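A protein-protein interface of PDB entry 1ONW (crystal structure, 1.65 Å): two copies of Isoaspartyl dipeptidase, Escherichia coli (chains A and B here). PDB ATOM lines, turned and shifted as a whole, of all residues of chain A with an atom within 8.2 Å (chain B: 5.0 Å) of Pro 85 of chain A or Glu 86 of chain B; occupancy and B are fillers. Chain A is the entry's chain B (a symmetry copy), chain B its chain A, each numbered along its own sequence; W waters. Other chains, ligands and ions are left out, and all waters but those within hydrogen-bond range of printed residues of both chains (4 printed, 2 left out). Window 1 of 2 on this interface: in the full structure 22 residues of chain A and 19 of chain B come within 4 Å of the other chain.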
ATOM      1  N   HIS A  70      -5.442  26.551  13.322  1.00  0.00           N
ATOM      2  CA  HIS A  70      -5.957  26.582  14.688  1.00  0.00           C
ATOM      3  C   HIS A  70      -6.934  25.428  14.895  1.00  0.00           C
ATOM      4  O   HIS A  70      -8.148  25.601  14.978  1.00  0.00           O
ATOM      5  CB  HIS A  70      -6.564  27.951  15.011  1.00  0.00           C
ATOM      6  CG  HIS A  70      -5.515  29.039  14.990  1.00  0.00           C
ATOM      7  ND1 HIS A  70      -4.903  29.470  16.156  1.00  0.00           N
ATOM      8  CD2 HIS A  70      -4.965  29.715  13.949  1.00  0.00           C
ATOM      9  CE1 HIS A  70      -4.049  30.430  15.822  1.00  0.00           C
ATOM     10  NE2 HIS A  70      -4.067  30.584  14.498  1.00  0.00           N
ATOM     11  N   LEU A  71      -6.358  24.218  14.956  1.00  0.00           N
ATOM     12  CA  LEU A  71      -7.092  22.975  15.073  1.00  0.00           C
ATOM     13  C   LEU A  71      -8.209  22.948  16.101  1.00  0.00           C
ATOM     14  O   LEU A  71      -9.244  22.364  15.812  1.00  0.00           O
ATOM     15  CB  LEU A  71      -6.205  21.736  15.322  1.00  0.00           C
ATOM     16  CG  LEU A  71      -5.118  21.531  14.261  1.00  0.00           C
ATOM     17  CD1 LEU A  71      -4.195  20.400  14.724  1.00  0.00           C
ATOM     18  CD2 LEU A  71      -5.762  21.157  12.928  1.00  0.00           C
ATOM     19  N   ILE A  72      -7.970  23.464  17.320  1.00  0.00           N
ATOM     20  CA  ILE A  72      -9.018  23.397  18.328  1.00  0.00           C
ATOM     21  C   ILE A  72      -9.951  24.601  18.314  1.00  0.00           C
ATOM     22  O   ILE A  72     -10.943  24.654  19.063  1.00  0.00           O
ATOM     23  CB  ILE A  72      -8.464  23.140  19.739  1.00  0.00           C
ATOM     24  CG1 ILE A  72      -7.472  24.226  20.126  1.00  0.00           C
ATOM     25  CG2 ILE A  72      -7.834  21.734  19.829  1.00  0.00           C
ATOM     26  CD1 ILE A  72      -7.197  24.265  21.622  1.00  0.00           C
ATOM     27  N   GLY A  73      -9.591  25.543  17.450  1.00  0.00           N
ATOM     28  CA  GLY A  73     -10.290  26.813  17.307  1.00  0.00           C
ATOM     29  C   GLY A  73      -9.368  27.911  17.834  1.00  0.00           C
ATOM     30  O   GLY A  73      -8.357  27.622  18.498  1.00  0.00           O
ATOM     31  N   GLY A  74      -9.689  29.176  17.521  1.00  0.00           N
ATOM     32  CA  GLY A  74      -8.876  30.308  17.948  1.00  0.00           C
ATOM     33  C   GLY A  74      -9.793  31.484  18.220  1.00  0.00           C
ATOM     34  O   GLY A  74     -10.862  31.326  18.781  1.00  0.00           O
ATOM     35  N   GLY A  75      -9.407  32.665  17.779  1.00  0.00           N
ATOM     36  CA  GLY A  75     -10.229  33.836  17.986  1.00  0.00           C
ATOM     37  C   GLY A  75     -10.315  34.162  19.483  1.00  0.00           C
ATOM     38  O   GLY A  75      -9.459  33.817  20.291  1.00  0.00           O
ATOM     39  N   PRO A  80     -15.665  36.252  24.376  1.00  0.00           N
ATOM     40  CA  PRO A  80     -15.866  34.830  24.253  1.00  0.00           C
ATOM     41  C   PRO A  80     -16.723  34.384  23.086  1.00  0.00           C
ATOM     42  O   PRO A  80     -16.641  33.217  22.679  1.00  0.00           O
ATOM     43  CB  PRO A  80     -16.424  34.332  25.580  1.00  0.00           C
ATOM     44  CG  PRO A  80     -16.805  35.569  26.367  1.00  0.00           C
ATOM     45  CD  PRO A  80     -16.064  36.738  25.712  1.00  0.00           C
ATOM     46  N   THR A  81     -17.567  35.287  22.572  1.00  0.00           N
ATOM     47  CA  THR A  81     -18.373  34.875  21.431  1.00  0.00           C
ATOM     48  C   THR A  81     -17.523  34.716  20.186  1.00  0.00           C
ATOM     49  O   THR A  81     -17.956  34.094  19.221  1.00  0.00           O
ATOM     50  CB  THR A  81     -19.558  35.817  21.126  1.00  0.00           C
ATOM     51  OG1 THR A  81     -19.034  37.026  20.643  1.00  0.00           O
ATOM     52  CG2 THR A  81     -20.368  36.070  22.388  1.00  0.00           C
ATOM     53  N   THR A  82     -16.319  35.284  20.179  1.00  0.00           N
ATOM     54  CA  THR A  82     -15.482  35.170  18.995  1.00  0.00           C
ATOM     55  C   THR A  82     -14.564  33.964  19.008  1.00  0.00           C
ATOM     56  O   THR A  82     -13.671  33.900  18.168  1.00  0.00           O
ATOM     57  CB  THR A  82     -14.713  36.460  18.669  1.00  0.00           C
ATOM     58  OG1 THR A  82     -13.832  36.795  19.738  1.00  0.00           O
ATOM     59  CG2 THR A  82     -15.729  37.585  18.514  1.00  0.00           C
ATOM     60  N   ARG A  83     -14.766  33.032  19.949  1.00  0.00           N
ATOM     61  CA  ARG A  83     -13.936  31.844  19.984  1.00  0.00           C
ATOM     62  C   ARG A  83     -14.452  30.897  18.932  1.00  0.00           C
ATOM     63  O   ARG A  83     -15.588  30.449  19.004  1.00  0.00           O
ATOM     64  CB  ARG A  83     -13.915  31.146  21.341  1.00  0.00           C
ATOM     65  CG  ARG A  83     -13.441  32.058  22.479  1.00  0.00           C
ATOM     66  CD  ARG A  83     -13.840  31.511  23.831  1.00  0.00           C
ATOM     67  NE  ARG A  83     -13.046  30.330  24.177  1.00  0.00           N
ATOM     68  CZ  ARG A  83     -13.460  29.055  24.236  1.00  0.00           C
ATOM     69  NH1 ARG A  83     -12.641  28.050  24.576  1.00  0.00           N
ATOM     70  NH2 ARG A  83     -14.718  28.752  23.957  1.00  0.00           N
ATOM     71  N   THR A  84     -13.617  30.594  17.948  1.00  0.00           N
ATOM     72  CA  THR A  84     -14.008  29.702  16.871  1.00  0.00           C
ATOM     73  C   THR A  84     -14.014  28.256  17.288  1.00  0.00           C
ATOM     74  O   THR A  84     -13.375  27.854  18.232  1.00  0.00           O
ATOM     75  CB  THR A  84     -13.171  29.910  15.601  1.00  0.00           C
ATOM     76  OG1 THR A  84     -11.799  29.746  15.939  1.00  0.00           O
ATOM     77  CG2 THR A  84     -13.401  31.329  15.101  1.00  0.00           C
ATOM     78  N   PRO A  85     -14.771  27.476  16.567  1.00  0.00           N
ATOM     79  CA  PRO A  85     -14.924  26.069  16.821  1.00  0.00           C
ATOM     80  C   PRO A  85     -13.749  25.270  16.255  1.00  0.00           C
ATOM     81  O   PRO A  85     -12.967  25.755  15.440  1.00  0.00           O
ATOM     82  CB  PRO A  85     -16.195  25.702  16.059  1.00  0.00           C
ATOM     83  CG  PRO A  85     -16.446  26.812  15.039  1.00  0.00           C
ATOM     84  CD  PRO A  85     -15.570  27.982  15.432  1.00  0.00           C
ATOM     85  N   GLU A  86     -13.615  24.043  16.723  1.00  0.00           N
ATOM     86  CA  GLU A  86     -12.555  23.170  16.251  1.00  0.00           C
ATOM     87  C   GLU A  86     -12.729  22.851  14.795  1.00  0.00           C
ATOM     88  O   GLU A  86     -13.830  22.855  14.267  1.00  0.00           O
ATOM     89  CB  GLU A  86     -12.568  21.850  17.033  1.00  0.00           C
ATOM     90  CG  GLU A  86     -13.609  20.837  16.551  1.00  0.00           C
ATOM     91  CD  GLU A  86     -13.720  19.704  17.551  1.00  0.00           C
ATOM     92  OE1 GLU A  86     -12.892  18.823  17.636  1.00  0.00           O
ATOM     93  OE2 GLU A  86     -14.756  19.787  18.355  1.00  0.00           O
ATOM     94  N   VAL A  87     -11.621  22.576  14.155  1.00  0.00           N
ATOM     95  CA  VAL A  87     -11.580  22.252  12.729  1.00  0.00           C
ATOM     96  C   VAL A  87     -12.188  20.877  12.423  1.00  0.00           C
ATOM     97  O   VAL A  87     -11.955  19.907  13.141  1.00  0.00           O
ATOM     98  CB  VAL A  87     -10.116  22.252  12.249  1.00  0.00           C
ATOM     99  CG1 VAL A  87      -9.912  21.367  11.026  1.00  0.00           C
ATOM    100  CG2 VAL A  87      -9.610  23.649  11.945  1.00  0.00           C
ATOM    101  N   ALA A  88     -12.948  20.785  11.327  1.00  0.00           N
ATOM    102  CA  ALA A  88     -13.512  19.517  10.884  1.00  0.00           C
ATOM    103  C   ALA A  88     -12.555  18.840   9.909  1.00  0.00           C
ATOM    104  O   ALA A  88     -11.966  19.497   9.066  1.00  0.00           O
ATOM    105  CB  ALA A  88     -14.825  19.761  10.154  1.00  0.00           C
ATOM    106  N   ARG A 111      -7.671  28.349  25.922  1.00  0.00           N
ATOM    107  CA  ARG A 111      -7.088  27.370  25.023  1.00  0.00           C
ATOM    108  C   ARG A 111      -5.820  26.798  25.671  1.00  0.00           C
ATOM    109  O   ARG A 111      -5.038  27.536  26.215  1.00  0.00           O
ATOM    110  CB  ARG A 111      -6.727  27.976  23.680  1.00  0.00           C
ATOM    111  CG  ARG A 111      -7.867  28.733  23.007  1.00  0.00           C
ATOM    112  CD  ARG A 111      -9.023  27.843  22.571  1.00  0.00           C
ATOM    113  NE  ARG A 111      -9.941  28.574  21.715  1.00  0.00           N
ATOM    114  CZ  ARG A 111     -11.015  28.030  21.167  1.00  0.00           C
ATOM    115  NH1 ARG A 111     -11.327  26.758  21.405  1.00  0.00           N
ATOM    116  NH2 ARG A 111     -11.789  28.782  20.378  1.00  0.00           N
ATOM    117  N   LYS A 119      -6.565  16.913  20.027  1.00  0.00           N
ATOM    118  CA  LYS A 119      -7.091  17.170  18.693  1.00  0.00           C
ATOM    119  C   LYS A 119      -6.148  16.667  17.602  1.00  0.00           C
ATOM    120  O   LYS A 119      -6.558  16.083  16.615  1.00  0.00           O
ATOM    121  CB  LYS A 119      -7.459  18.643  18.490  1.00  0.00           C
ATOM    122  CG  LYS A 119      -8.029  18.925  17.078  1.00  0.00           C
ATOM    123  CD  LYS A 119      -9.384  18.285  16.726  1.00  0.00           C
ATOM    124  CE  LYS A 119     -10.005  18.762  15.424  1.00  0.00           C
ATOM    125  NZ  LYS A 119     -11.352  18.220  15.130  1.00  0.00           N
ATOM    126  N   GLY A 286      -5.783  28.863   9.074  1.00  0.00           N
ATOM    127  CA  GLY A 286      -7.151  28.398   9.049  1.00  0.00           C
ATOM    128  C   GLY A 286      -7.747  28.207  10.425  1.00  0.00           C
ATOM    129  O   GLY A 286      -7.040  27.948  11.408  1.00  0.00           O
ATOM    130  N   ASN A 287      -9.076  28.350  10.447  1.00  0.00           N
ATOM    131  CA  ASN A 287      -9.857  28.138  11.644  1.00  0.00           C
ATOM    132  C   ASN A 287      -9.773  29.227  12.701  1.00  0.00           C
ATOM    133  O   ASN A 287     -10.301  29.091  13.800  1.00  0.00           O
ATOM    134  CB  ASN A 287      -9.656  26.721  12.204  1.00  0.00           C
ATOM    135  CG  ASN A 287     -10.904  26.160  12.851  1.00  0.00           C
ATOM    136  OD1 ASN A 287     -11.974  26.213  12.237  1.00  0.00           O
ATOM    137  ND2 ASN A 287     -10.778  25.602  14.070  1.00  0.00           N
ATOM    138  N   GLY A 288      -9.115  30.306  12.362  1.00  0.00           N
ATOM    139  CA  GLY A 288      -9.052  31.454  13.233  1.00  0.00           C
ATOM    140  C   GLY A 288     -10.298  32.273  12.880  1.00  0.00           C
ATOM    141  O   GLY A 288     -11.129  31.828  12.064  1.00  0.00           O
ATOM    142  N   SER A 289     -10.455  33.452  13.480  1.00  0.00           N
ATOM    143  CA  SER A 289     -11.615  34.283  13.192  1.00  0.00           C
ATOM    144  C   SER A 289     -11.339  35.206  12.008  1.00  0.00           C
ATOM    145  O   SER A 289     -10.226  35.696  11.809  1.00  0.00           O
ATOM    146  CB  SER A 289     -12.219  35.022  14.390  1.00  0.00           C
ATOM    147  OG  SER A 289     -11.268  35.899  14.955  1.00  0.00           O
ATOM    148  N   GLY A 303     -16.512  35.474  10.810  1.00  0.00           N
ATOM    149  CA  GLY A 303     -16.536  34.085  10.296  1.00  0.00           C
ATOM    150  C   GLY A 303     -15.274  33.276  10.646  1.00  0.00           C
ATOM    151  O   GLY A 303     -14.368  33.747  11.331  1.00  0.00           O
ATOM    152  N   VAL A 304     -15.222  32.030  10.187  1.00  0.00           N
ATOM    153  CA  VAL A 304     -14.070  31.169  10.449  1.00  0.00           C
ATOM    154  C   VAL A 304     -13.156  31.203   9.226  1.00  0.00           C
ATOM    155  O   VAL A 304     -13.631  31.076   8.102  1.00  0.00           O
ATOM    156  CB  VAL A 304     -14.557  29.732  10.668  1.00  0.00           C
ATOM    157  CG1 VAL A 304     -13.435  28.865  11.218  1.00  0.00           C
ATOM    158  CG2 VAL A 304     -15.748  29.699  11.625  1.00  0.00           C
ATOM    159  N   ALA A 305     -11.857  31.387   9.379  1.00  0.00           N
ATOM    160  CA  ALA A 305     -11.070  31.383   8.163  1.00  0.00           C
ATOM    161  C   ALA A 305     -11.031  29.954   7.652  1.00  0.00           C
ATOM    162  O   ALA A 305     -10.932  29.007   8.440  1.00  0.00           O
ATOM    163  CB  ALA A 305      -9.685  31.972   8.357  1.00  0.00           C
ATOM    164  N   LEU B  71     -21.223  21.715  27.686  1.00  0.00           N
ATOM    165  CA  LEU B  71     -21.169  22.910  26.833  1.00  0.00           C
ATOM    166  C   LEU B  71     -19.988  22.987  25.857  1.00  0.00           C
ATOM    167  O   LEU B  71     -20.133  23.441  24.740  1.00  0.00           O
ATOM    168  CB  LEU B  71     -21.166  24.200  27.694  1.00  0.00           C
ATOM    169  CG  LEU B  71     -22.444  24.459  28.495  1.00  0.00           C
ATOM    170  CD1 LEU B  71     -22.300  25.792  29.217  1.00  0.00           C
ATOM    171  CD2 LEU B  71     -23.608  24.554  27.522  1.00  0.00           C
ATOM    172  N   ILE B  72     -18.788  22.624  26.319  1.00  0.00           N
ATOM    173  CA  ILE B  72     -17.621  22.735  25.466  1.00  0.00           C
ATOM    174  C   ILE B  72     -17.323  21.434  24.755  1.00  0.00           C
ATOM    175  O   ILE B  72     -16.349  21.375  23.986  1.00  0.00           O
ATOM    176  CB  ILE B  72     -16.343  23.174  26.208  1.00  0.00           C
ATOM    177  CG1 ILE B  72     -15.919  22.218  27.327  1.00  0.00           C
ATOM    178  CG2 ILE B  72     -16.422  24.603  26.704  1.00  0.00           C
ATOM    179  CD1 ILE B  72     -14.499  22.469  27.849  1.00  0.00           C
ATOM    180  N   GLY B  73     -18.144  20.413  25.009  1.00  0.00           N
ATOM    181  CA  GLY B  73     -17.888  19.123  24.406  1.00  0.00           C
ATOM    182  C   GLY B  73     -17.455  18.209  25.528  1.00  0.00           C
ATOM    183  O   GLY B  73     -17.079  18.685  26.604  1.00  0.00           O
ATOM    184  N   THR B  84     -16.366  15.137  21.977  1.00  0.00           N
ATOM    185  CA  THR B  84     -17.438  15.785  21.249  1.00  0.00           C
ATOM    186  C   THR B  84     -17.203  17.253  21.142  1.00  0.00           C
ATOM    187  O   THR B  84     -16.438  17.871  21.870  1.00  0.00           O
ATOM    188  CB  THR B  84     -18.831  15.543  21.841  1.00  0.00           C
ATOM    189  OG1 THR B  84     -18.801  16.005  23.170  1.00  0.00           O
ATOM    190  CG2 THR B  84     -19.176  14.062  21.802  1.00  0.00           C
ATOM    191  N   PRO B  85     -17.921  17.779  20.201  1.00  0.00           N
ATOM    192  CA  PRO B  85     -17.894  19.176  19.854  1.00  0.00           C
ATOM    193  C   PRO B  85     -18.660  20.054  20.860  1.00  0.00           C
ATOM    194  O   PRO B  85     -19.506  19.587  21.629  1.00  0.00           O
ATOM    195  CB  PRO B  85     -18.583  19.226  18.469  1.00  0.00           C
ATOM    196  CG  PRO B  85     -19.163  17.843  18.154  1.00  0.00           C
ATOM    197  CD  PRO B  85     -18.583  16.902  19.188  1.00  0.00           C
ATOM    198  N   GLU B  86     -18.336  21.348  20.855  1.00  0.00           N
ATOM    199  CA  GLU B  86     -19.008  22.279  21.735  1.00  0.00           C
ATOM    200  C   GLU B  86     -20.475  22.422  21.311  1.00  0.00           C
ATOM    201  O   GLU B  86     -20.828  22.166  20.148  1.00  0.00           O
ATOM    202  CB  GLU B  86     -18.301  23.652  21.722  1.00  0.00           C
ATOM    203  CG  GLU B  86     -18.551  24.433  20.417  1.00  0.00           C
ATOM    204  CD  GLU B  86     -17.839  25.751  20.369  1.00  0.00           C
ATOM    205  OE1 GLU B  86     -18.279  26.788  20.830  1.00  0.00           O
ATOM    206  OE2 GLU B  86     -16.685  25.660  19.774  1.00  0.00           O
ATOM    207  N   VAL B  87     -21.335  22.826  22.238  1.00  0.00           N
ATOM    208  CA  VAL B  87     -22.750  22.967  21.896  1.00  0.00           C
ATOM    209  C   VAL B  87     -23.016  24.227  21.116  1.00  0.00           C
ATOM    210  O   VAL B  87     -22.366  25.265  21.309  1.00  0.00           O
ATOM    211  CB  VAL B  87     -23.693  22.943  23.097  1.00  0.00           C
ATOM    212  CG1 VAL B  87     -23.581  21.629  23.857  1.00  0.00           C
ATOM    213  CG2 VAL B  87     -23.435  24.152  23.993  1.00  0.00           C
ATOM    214  N   ALA B  88     -24.023  24.100  20.247  1.00  0.00           N
ATOM    215  CA  ALA B  88     -24.504  25.205  19.428  1.00  0.00           C
ATOM    216  C   ALA B  88     -25.743  25.841  20.056  1.00  0.00           C
ATOM    217  O   ALA B  88     -26.674  25.164  20.484  1.00  0.00           O
ATOM    218  CB  ALA B  88     -24.823  24.775  18.010  1.00  0.00           C
ATOM    219  N   LYS B 119     -17.047  29.499  27.375  1.00  0.00           N
ATOM    220  CA  LYS B 119     -18.232  29.142  26.598  1.00  0.00           C
ATOM    221  C   LYS B 119     -19.497  29.574  27.318  1.00  0.00           C
ATOM    222  O   LYS B 119     -20.459  30.028  26.727  1.00  0.00           O
ATOM    223  CB  LYS B 119     -18.241  27.634  26.338  1.00  0.00           C
ATOM    224  CG  LYS B 119     -19.476  27.148  25.567  1.00  0.00           C
ATOM    225  CD  LYS B 119     -19.524  27.566  24.101  1.00  0.00           C
ATOM    226  CE  LYS B 119     -20.646  26.854  23.355  1.00  0.00           C
ATOM    227  NZ  LYS B 119     -20.857  27.359  21.984  1.00  0.00           N
ATOM    228  N   ASN B 287     -24.744  16.839  24.677  1.00  0.00           N
ATOM    229  CA  ASN B 287     -23.457  17.140  24.124  1.00  0.00           C
ATOM    230  C   ASN B 287     -22.386  16.206  24.597  1.00  0.00           C
ATOM    231  O   ASN B 287     -21.214  16.350  24.280  1.00  0.00           O
ATOM    232  CB  ASN B 287     -23.053  18.603  24.280  1.00  0.00           C
ATOM    233  CG  ASN B 287     -22.258  19.065  23.095  1.00  0.00           C
ATOM    234  OD1 ASN B 287     -22.759  19.020  21.976  1.00  0.00           O
ATOM    235  ND2 ASN B 287     -21.052  19.572  23.343  1.00  0.00           N
ATOM    236  N   PHE B 387     -20.744  31.479  15.205  1.00  0.00           N
ATOM    237  CA  PHE B 387     -20.195  30.673  14.126  1.00  0.00           C
ATOM    238  C   PHE B 387     -21.085  29.594  13.579  1.00  0.00           C
ATOM    239  O   PHE B 387     -20.590  28.704  12.877  1.00  0.00           O
ATOM    240  CB  PHE B 387     -18.835  30.074  14.483  1.00  0.00           C
ATOM    241  CG  PHE B 387     -17.894  31.211  14.764  1.00  0.00           C
ATOM    242  CD1 PHE B 387     -17.406  31.461  16.050  1.00  0.00           C
ATOM    243  CD2 PHE B 387     -17.531  32.058  13.720  1.00  0.00           C
ATOM    244  CE1 PHE B 387     -16.568  32.551  16.322  1.00  0.00           C
ATOM    245  CE2 PHE B 387     -16.684  33.142  13.963  1.00  0.00           C
ATOM    246  CZ  PHE B 387     -16.208  33.379  15.260  1.00  0.00           C
HETATM  247  O   HOH W   1     -15.662  22.978  18.946  1.00  0.00           O
HETATM  248  O   HOH W   2     -15.942  26.222  23.263  1.00  0.00           O
HETATM  249  O   HOH W   3     -14.073  26.211  20.133  1.00  0.00           O
HETATM  250  O   HOH W   4     -17.744  29.551  20.736  1.00  0.00           O
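Thr 81 of chain A touches Phe 387 of chain B.
Thr 82 of chain A touches Phe 387 of chain B (C to CE1, 3.6 Å).
Arg 83 of chain A touches Phe 387 of chain B (O to CE1, 3.5 Å).
CZ of Phe 387 of chain B touches CG2 of Thr 84 of chain A (3.5 Å).
Glu 86 of chain B touches Pro 85 of chain A.
Phe 387 of chain B touches Pro 85 of chain A.
Glu 86 of chain A touches Pro 85 of chain B (OE2 to CA, 3.5 Å).
Phe 387 of chain B touches Gly 303 of chain A.
CG2 of Val 304 of chain A touches CD2 of Phe 387 of chain B, at 3.6 Å.
Printed residues of chain B that touch a printed residue of chain A: Pro 85, Glu 86 and Phe 387.
Hydrophobic or aromatic side chains of chain B within 4 Å of the printed part of chain A: Pro 85 and Phe 387.
Along chain A the printed residues that touch a printed residue of chain B span positions 81 to 304.
Among the printed residues, no Asp or Glu carboxylate lies within 4 Å of a Lys or Arg side-chain nitrogen of the other chain.
Pro 85 of chain A touches Glu 86 of chain B, and with the chains exchanged Glu 86 of chain A touches Pro 85 of chain B.
Of the 9 pairs that touch across the chains among the printed residues, 2 have their exchanged pair printed and touching as well.
OD1 of Asn 287 of chain B sits close to O of Pro 85 of chain B (3.3 Å).
The side-chain amino group (NZ) of Lys 119 of chain B lies within salt-bridge range of the side-chain carboxylate (OE1) of Glu 86 of chain B (2.9 Å).
The backbone carbonyl oxygen (O) of Thr 84 of chain A sits at hydrogen-bond distance from the guanidinium group (NH2) of Arg 111 of chain A, at 2.8 Å.
O of Asn 287 of chain A is in hydrogen-bond range of OG1 of Thr 84 of chain A (2.7 Å).
ND2 of Asn 287 of chain A is in hydrogen-bond range of O of Pro 85 of chain A.
OE1 of Glu 86 of chain A is in salt-bridge range of NZ of Lys 119 of chain A.
Printed residues of chain B within 4 Å of Glu 86 of chain A: Pro 85.
Of the printed residues of chain B, Gly 303 of chain A touches Phe 387.
Leu 71 of chain B touches none of the printed residues of chain A.
Printed residues of chain A within 4 Å of Pro 85 of chain B: Glu 86 (3.5 Å).
The nearest printed residue of chain B that does not touch Pro 85 of chain A is Pro 85 of chain B (7.3 Å).
Water W3 lies within hydrogen-bond range of the backbone carbonyl oxygen of Thr 84 of chain A (2.6 Å), the side-chain carboxylate of Glu 86 of chain B (2.7 Å) and the guanidinium group of Arg 111 of chain A (3.1 Å).
Water W4 lies within hydrogen-bond range of the side-chain carboxylate (OE1) of Glu 86 of chain B (2.8 Å) and the backbone carbonyl oxygen (O) of Arg 83 of chain A (2.9 Å).
Water W2 lies within hydrogen-bond range of NH2 of Arg 83 of chain A and OE1 of Glu 86 of chain B.
Water W1 bridges the side-chain carboxylate (OE2) of Glu 86 of chain B (3.0 Å) and the backbone NH (N) of Glu 86 of chain A (3.2 Å).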
